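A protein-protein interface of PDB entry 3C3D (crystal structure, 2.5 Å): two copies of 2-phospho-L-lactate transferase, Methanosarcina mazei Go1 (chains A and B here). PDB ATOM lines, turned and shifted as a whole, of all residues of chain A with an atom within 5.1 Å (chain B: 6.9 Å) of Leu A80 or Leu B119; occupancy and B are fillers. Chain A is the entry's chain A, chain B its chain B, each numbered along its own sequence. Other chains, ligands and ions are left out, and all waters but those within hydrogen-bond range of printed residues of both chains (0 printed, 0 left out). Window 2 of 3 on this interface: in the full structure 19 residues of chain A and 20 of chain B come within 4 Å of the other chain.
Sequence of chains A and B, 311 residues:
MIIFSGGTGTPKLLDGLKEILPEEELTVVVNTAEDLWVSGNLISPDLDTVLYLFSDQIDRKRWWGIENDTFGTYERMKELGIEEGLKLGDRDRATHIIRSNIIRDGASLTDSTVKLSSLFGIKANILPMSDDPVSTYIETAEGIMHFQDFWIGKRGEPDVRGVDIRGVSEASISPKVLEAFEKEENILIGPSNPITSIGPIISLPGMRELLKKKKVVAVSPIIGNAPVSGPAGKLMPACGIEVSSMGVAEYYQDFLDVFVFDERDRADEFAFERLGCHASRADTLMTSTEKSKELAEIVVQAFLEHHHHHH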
ATOM      1  N   ARG A  76      -2.443 -33.996  20.542  1.00  0.00           N
ATOM      2  CA  ARG A  76      -3.192 -32.786  20.816  1.00  0.00           C
ATOM      3  C   ARG A  76      -2.925 -31.757  19.718  1.00  0.00           C
ATOM      4  O   ARG A  76      -3.854 -31.170  19.172  1.00  0.00           O
ATOM      5  CB  ARG A  76      -2.807 -32.218  22.183  1.00  0.00           C
ATOM      6  CG  ARG A  76      -3.485 -30.904  22.527  1.00  0.00           C
ATOM      7  CD  ARG A  76      -4.993 -30.964  22.296  1.00  0.00           C
ATOM      8  NE  ARG A  76      -5.624 -29.676  22.567  1.00  0.00           N
ATOM      9  CZ  ARG A  76      -6.785 -29.282  22.049  1.00  0.00           C
ATOM     10  NH1 ARG A  76      -7.276 -28.091  22.360  1.00  0.00           N
ATOM     11  NH2 ARG A  76      -7.447 -30.069  21.213  1.00  0.00           N
ATOM     12  N   MET A  77      -1.661 -31.554  19.379  1.00  0.00           N
ATOM     13  CA  MET A  77      -1.312 -30.590  18.345  1.00  0.00           C
ATOM     14  C   MET A  77      -1.812 -30.997  16.966  1.00  0.00           C
ATOM     15  O   MET A  77      -2.070 -30.148  16.115  1.00  0.00           O
ATOM     16  CB  MET A  77       0.198 -30.382  18.314  1.00  0.00           C
ATOM     17  CG  MET A  77       0.679 -29.513  19.450  1.00  0.00           C
ATOM     18  SD  MET A  77       2.582 -29.583  19.699  1.00  0.00           S
ATOM     19  CE  MET A  77       3.110 -28.278  18.370  1.00  0.00           C
ATOM     20  N   LYS A  78      -1.952 -32.299  16.752  1.00  0.00           N
ATOM     21  CA  LYS A  78      -2.431 -32.799  15.475  1.00  0.00           C
ATOM     22  C   LYS A  78      -3.909 -32.423  15.331  1.00  0.00           C
ATOM     23  O   LYS A  78      -4.350 -32.022  14.259  1.00  0.00           O
ATOM     24  CB  LYS A  78      -2.241 -34.317  15.395  1.00  0.00           C
ATOM     25  CG  LYS A  78      -2.382 -34.866  13.984  1.00  0.00           C
ATOM     26  CD  LYS A  78      -1.802 -36.276  13.819  1.00  0.00           C
ATOM     27  CE  LYS A  78      -2.686 -37.366  14.426  1.00  0.00           C
ATOM     28  NZ  LYS A  78      -2.837 -37.267  15.916  1.00  0.00           N
ATOM     29  N   GLU A  79      -4.661 -32.546  16.423  1.00  0.00           N
ATOM     30  CA  GLU A  79      -6.078 -32.203  16.425  1.00  0.00           C
ATOM     31  C   GLU A  79      -6.242 -30.727  16.072  1.00  0.00           C
ATOM     32  O   GLU A  79      -7.254 -30.334  15.489  1.00  0.00           O
ATOM     33  CB  GLU A  79      -6.688 -32.442  17.809  1.00  0.00           C
ATOM     34  CG  GLU A  79      -6.599 -33.862  18.310  1.00  0.00           C
ATOM     35  CD  GLU A  79      -7.053 -34.004  19.766  1.00  0.00           C
ATOM     36  OE1 GLU A  79      -7.108 -35.157  20.261  1.00  0.00           O
ATOM     37  OE2 GLU A  79      -7.349 -32.973  20.415  1.00  0.00           O
ATOM     38  N   LEU A  80      -5.247 -29.919  16.441  1.00  0.00           N
ATOM     39  CA  LEU A  80      -5.259 -28.483  16.184  1.00  0.00           C
ATOM     40  C   LEU A  80      -4.606 -28.153  14.852  1.00  0.00           C
ATOM     41  O   LEU A  80      -4.513 -26.987  14.462  1.00  0.00           O
ATOM     42  CB  LEU A  80      -4.534 -27.743  17.311  1.00  0.00           C
ATOM     43  CG  LEU A  80      -5.287 -27.294  18.573  1.00  0.00           C
ATOM     44  CD1 LEU A  80      -6.445 -28.197  18.897  1.00  0.00           C
ATOM     45  CD2 LEU A  80      -4.301 -27.253  19.726  1.00  0.00           C
ATOM     46  N   GLY A  81      -4.139 -29.191  14.164  1.00  0.00           N
ATOM     47  CA  GLY A  81      -3.511 -29.008  12.868  1.00  0.00           C
ATOM     48  C   GLY A  81      -2.127 -28.395  12.887  1.00  0.00           C
ATOM     49  O   GLY A  81      -1.759 -27.666  11.965  1.00  0.00           O
ATOM     50  N   ILE A  82      -1.354 -28.682  13.928  1.00  0.00           N
ATOM     51  CA  ILE A  82       0.000 -28.155  14.035  1.00  0.00           C
ATOM     52  C   ILE A  82       0.981 -29.323  14.040  1.00  0.00           C
ATOM     53  O   ILE A  82       0.864 -30.232  14.852  1.00  0.00           O
ATOM     54  CB  ILE A  82       0.178 -27.345  15.332  1.00  0.00           C
ATOM     55  CG1 ILE A  82      -0.873 -26.235  15.406  1.00  0.00           C
ATOM     56  CG2 ILE A  82       1.577 -26.768  15.386  1.00  0.00           C
ATOM     57  CD1 ILE A  82      -0.862 -25.283  14.219  1.00  0.00           C
ATOM     58  N   ARG B  91      -1.320 -32.336  27.238  1.00  0.00           N
ATOM     59  CA  ARG B  91      -2.118 -31.452  26.395  1.00  0.00           C
ATOM     60  C   ARG B  91      -1.811 -29.998  26.728  1.00  0.00           C
ATOM     61  O   ARG B  91      -1.736 -29.138  25.843  1.00  0.00           O
ATOM     62  CB  ARG B  91      -3.611 -31.754  26.578  1.00  0.00           C
ATOM     63  CG  ARG B  91      -4.000 -33.155  26.095  1.00  0.00           C
ATOM     64  CD  ARG B  91      -5.436 -33.529  26.449  1.00  0.00           C
ATOM     65  NE  ARG B  91      -6.412 -32.858  25.599  1.00  0.00           N
ATOM     66  CZ  ARG B  91      -6.611 -33.139  24.312  1.00  0.00           C
ATOM     67  NH1 ARG B  91      -7.525 -32.467  23.623  1.00  0.00           N
ATOM     68  NH2 ARG B  91      -5.905 -34.098  23.716  1.00  0.00           N
ATOM     69  N   ALA B  94       1.202 -28.654  24.967  1.00  0.00           N
ATOM     70  CA  ALA B  94       0.987 -28.286  23.573  1.00  0.00           C
ATOM     71  C   ALA B  94       0.750 -26.783  23.448  1.00  0.00           C
ATOM     72  O   ALA B  94       1.289 -26.131  22.542  1.00  0.00           O
ATOM     73  CB  ALA B  94      -0.193 -29.062  22.993  1.00  0.00           C
ATOM     74  N   THR B  95      -0.033 -26.233  24.370  1.00  0.00           N
ATOM     75  CA  THR B  95      -0.328 -24.804  24.386  1.00  0.00           C
ATOM     76  C   THR B  95       0.972 -23.999  24.541  1.00  0.00           C
ATOM     77  O   THR B  95       1.192 -23.009  23.839  1.00  0.00           O
ATOM     78  CB  THR B  95      -1.277 -24.456  25.569  1.00  0.00           C
ATOM     79  OG1 THR B  95      -2.464 -25.249  25.468  1.00  0.00           O
ATOM     80  CG2 THR B  95      -1.655 -22.975  25.556  1.00  0.00           C
ATOM     81  N   ILE B  98       2.935 -24.348  21.178  1.00  0.00           N
ATOM     82  CA  ILE B  98       2.353 -23.558  20.095  1.00  0.00           C
ATOM     83  C   ILE B  98       2.631 -22.069  20.321  1.00  0.00           C
ATOM     84  O   ILE B  98       3.003 -21.348  19.395  1.00  0.00           O
ATOM     85  CB  ILE B  98       0.830 -23.806  19.979  1.00  0.00           C
ATOM     86  CG1 ILE B  98       0.579 -25.256  19.566  1.00  0.00           C
ATOM     87  CG2 ILE B  98       0.212 -22.878  18.945  1.00  0.00           C
ATOM     88  CD1 ILE B  98      -0.866 -25.667  19.694  1.00  0.00           C
ATOM     89  N   ILE B 102       5.579 -19.612  18.106  1.00  0.00           N
ATOM     90  CA  ILE B 102       5.200 -18.343  17.507  1.00  0.00           C
ATOM     91  C   ILE B 102       6.144 -17.247  17.991  1.00  0.00           C
ATOM     92  O   ILE B 102       6.590 -16.415  17.207  1.00  0.00           O
ATOM     93  CB  ILE B 102       3.738 -17.986  17.846  1.00  0.00           C
ATOM     94  CG1 ILE B 102       2.802 -18.922  17.078  1.00  0.00           C
ATOM     95  CG2 ILE B 102       3.449 -16.538  17.496  1.00  0.00           C
ATOM     96  CD1 ILE B 102       1.357 -18.806  17.489  1.00  0.00           C
ATOM     97  N   SER B 112       0.636 -14.799  19.686  1.00  0.00           N
ATOM     98  CA  SER B 112       0.416 -16.205  20.017  1.00  0.00           C
ATOM     99  C   SER B 112      -0.942 -16.404  20.689  1.00  0.00           C
ATOM    100  O   SER B 112      -1.617 -17.412  20.450  1.00  0.00           O
ATOM    101  CB  SER B 112       1.527 -16.730  20.938  1.00  0.00           C
ATOM    102  OG  SER B 112       1.469 -16.119  22.214  1.00  0.00           O
ATOM    103  N   VAL B 114      -3.658 -14.597  20.238  1.00  0.00           N
ATOM    104  CA  VAL B 114      -4.684 -14.444  19.218  1.00  0.00           C
ATOM    105  C   VAL B 114      -4.790 -15.739  18.408  1.00  0.00           C
ATOM    106  O   VAL B 114      -5.894 -16.203  18.100  1.00  0.00           O
ATOM    107  CB  VAL B 114      -4.359 -13.249  18.278  1.00  0.00           C
ATOM    108  CG1 VAL B 114      -5.309 -13.231  17.087  1.00  0.00           C
ATOM    109  CG2 VAL B 114      -4.467 -11.946  19.056  1.00  0.00           C
ATOM    110  N   LYS B 115      -3.644 -16.328  18.077  1.00  0.00           N
ATOM    111  CA  LYS B 115      -3.609 -17.576  17.314  1.00  0.00           C
ATOM    112  C   LYS B 115      -4.214 -18.718  18.121  1.00  0.00           C
ATOM    113  O   LYS B 115      -5.047 -19.487  17.622  1.00  0.00           O
ATOM    114  CB  LYS B 115      -2.167 -17.917  16.943  1.00  0.00           C
ATOM    115  CG  LYS B 115      -1.998 -19.227  16.194  1.00  0.00           C
ATOM    116  CD  LYS B 115      -2.634 -19.167  14.825  1.00  0.00           C
ATOM    117  CE  LYS B 115      -2.394 -20.452  14.054  1.00  0.00           C
ATOM    118  NZ  LYS B 115      -3.093 -20.434  12.742  1.00  0.00           N
ATOM    119  N   LEU B 116      -3.793 -18.837  19.374  1.00  0.00           N
ATOM    120  CA  LEU B 116      -4.315 -19.881  20.236  1.00  0.00           C
ATOM    121  C   LEU B 116      -5.832 -19.740  20.337  1.00  0.00           C
ATOM    122  O   LEU B 116      -6.556 -20.736  20.349  1.00  0.00           O
ATOM    123  CB  LEU B 116      -3.669 -19.793  21.621  1.00  0.00           C
ATOM    124  CG  LEU B 116      -2.282 -20.441  21.710  1.00  0.00           C
ATOM    125  CD1 LEU B 116      -1.611 -20.057  23.015  1.00  0.00           C
ATOM    126  CD2 LEU B 116      -2.424 -21.958  21.586  1.00  0.00           C
ATOM    127  N   SER B 117      -6.316 -18.504  20.392  1.00  0.00           N
ATOM    128  CA  SER B 117      -7.752 -18.284  20.466  1.00  0.00           C
ATOM    129  C   SER B 117      -8.450 -18.818  19.223  1.00  0.00           C
ATOM    130  O   SER B 117      -9.548 -19.373  19.322  1.00  0.00           O
ATOM    131  CB  SER B 117      -8.059 -16.800  20.638  1.00  0.00           C
ATOM    132  OG  SER B 117      -7.676 -16.371  21.930  1.00  0.00           O
ATOM    133  N   SER B 118      -7.828 -18.660  18.056  1.00  0.00           N
ATOM    134  CA  SER B 118      -8.435 -19.176  16.837  1.00  0.00           C
ATOM    135  C   SER B 118      -8.392 -20.692  16.858  1.00  0.00           C
ATOM    136  O   SER B 118      -9.378 -21.346  16.521  1.00  0.00           O
ATOM    137  CB  SER B 118      -7.697 -18.695  15.587  1.00  0.00           C
ATOM    138  OG  SER B 118      -7.597 -17.288  15.572  1.00  0.00           O
ATOM    139  N   LEU B 119      -7.247 -21.253  17.237  1.00  0.00           N
ATOM    140  CA  LEU B 119      -7.119 -22.706  17.285  1.00  0.00           C
ATOM    141  C   LEU B 119      -8.135 -23.306  18.236  1.00  0.00           C
ATOM    142  O   LEU B 119      -8.693 -24.366  17.971  1.00  0.00           O
ATOM    143  CB  LEU B 119      -5.715 -23.113  17.729  1.00  0.00           C
ATOM    144  CG  LEU B 119      -4.568 -22.687  16.818  1.00  0.00           C
ATOM    145  CD1 LEU B 119      -3.240 -22.932  17.521  1.00  0.00           C
ATOM    146  CD2 LEU B 119      -4.644 -23.452  15.507  1.00  0.00           C
ATOM    147  N   PHE B 120      -8.371 -22.630  19.351  1.00  0.00           N
ATOM    148  CA  PHE B 120      -9.322 -23.121  20.338  1.00  0.00           C
ATOM    149  C   PHE B 120     -10.775 -22.771  20.014  1.00  0.00           C
ATOM    150  O   PHE B 120     -11.683 -23.195  20.728  1.00  0.00           O
ATOM    151  CB  PHE B 120      -8.971 -22.573  21.722  1.00  0.00           C
ATOM    152  CG  PHE B 120      -7.725 -23.174  22.320  1.00  0.00           C
ATOM    153  CD1 PHE B 120      -7.268 -22.741  23.560  1.00  0.00           C
ATOM    154  CD2 PHE B 120      -7.032 -24.188  21.665  1.00  0.00           C
ATOM    155  CE1 PHE B 120      -6.148 -23.309  24.145  1.00  0.00           C
ATOM    156  CE2 PHE B 120      -5.908 -24.765  22.240  1.00  0.00           C
ATOM    157  CZ  PHE B 120      -5.465 -24.323  23.488  1.00  0.00           C
ATOM    158  N   GLY B 121     -10.993 -21.999  18.953  1.00  0.00           N
ATOM    159  CA  GLY B 121     -12.339 -21.613  18.585  1.00  0.00           C
ATOM    160  C   GLY B 121     -12.962 -20.646  19.581  1.00  0.00           C
ATOM    161  O   GLY B 121     -14.156 -20.707  19.855  1.00  0.00           O
ATOM    162  N   ILE B 122     -12.161 -19.740  20.124  1.00  0.00           N
ATOM    163  CA  ILE B 122     -12.660 -18.782  21.102  1.00  0.00           C
ATOM    164  C   ILE B 122     -13.055 -17.461  20.432  1.00  0.00           C
ATOM    165  O   ILE B 122     -12.340 -16.975  19.561  1.00  0.00           O
ATOM    166  CB  ILE B 122     -11.580 -18.549  22.188  1.00  0.00           C
ATOM    167  CG1 ILE B 122     -11.421 -19.833  23.011  1.00  0.00           C
ATOM    168  CG2 ILE B 122     -11.935 -17.358  23.071  1.00  0.00           C
ATOM    169  CD1 ILE B 122     -10.099 -19.937  23.723  1.00  0.00           C
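Hydrophobic or aromatic side chains of chain A within 4 Å of the printed part of chain B: Met A77 and Leu A80. Of the 15 printed residues of chain B, 5 touch a printed residue of chain A. Printed residues of chain B that touch a printed residue of chain A: Arg B91, Ala B94, Ile B98, Leu B119 and Phe B120. Hydrophobic or aromatic side chains of chain B that line the printed part of chain A: Ala B94, Ile B98, Leu B119 and Phe B120. Among the printed residues, Asp or Glu carboxylates within 4 Å of a Lys or Arg side-chain nitrogen of the other chain: Glu A79 with Arg B91.
No position is printed for both chains. Of the 8 pairs that touch across the chains among the printed residues, none has its exchanged pair printed and touching as well.
Among the printed residues, pairs that only touch across the chains: Arg A76 with Phe B120 (3.6 Å), Met A77 with Ala B94 (3.7 Å), Leu A80 with Leu B119 (3.7 Å), Leu A80 with Ile B98 (3.8 Å), Arg A76 with Ala B94 (3.8 Å) and Leu A80 with Phe B120 (3.9 Å).
The guanidinium group (NH1) of Arg B91 sits close to the guanidinium group (NH2) of Arg A76, at 3.4 Å. NH1 of Arg B91 lies within salt-bridge range of OE2 of Glu A79 (3.3 Å).
N of Ile A82 sits at hydrogen-bond distance from O of Met A77 (2.7 Å). The side-chain carboxylate of Glu A79 is in salt-bridge range of the guanidinium group of Arg A76, 3.0 Å away.
Printed residues of chain B within 4 Å of Leu A80: Ile B98, Leu B119 and Phe B120. Leu B119 touches just one residue of chain A: Leu A80 (3.7 Å). Of the printed residues of chain A, Ala B94 touches Arg A76 (3.8 Å) and Met A77 (3.7 Å). Of the printed residues of chain B, Met A77 touches Ala B94. Of the printed residues of chain B, Glu A79 touches Arg B91 (3.3 Å). Of the printed residues of chain A, Arg B91 touches Arg A76 (3.2 Å) and Glu A79 (3.3 Å). Printed residues of chain A within 4 Å of Phe B120: Arg A76 and Leu A80. The nearest residue of chain B that does not touch Leu A80 is Ala B94 (5.6 Å).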
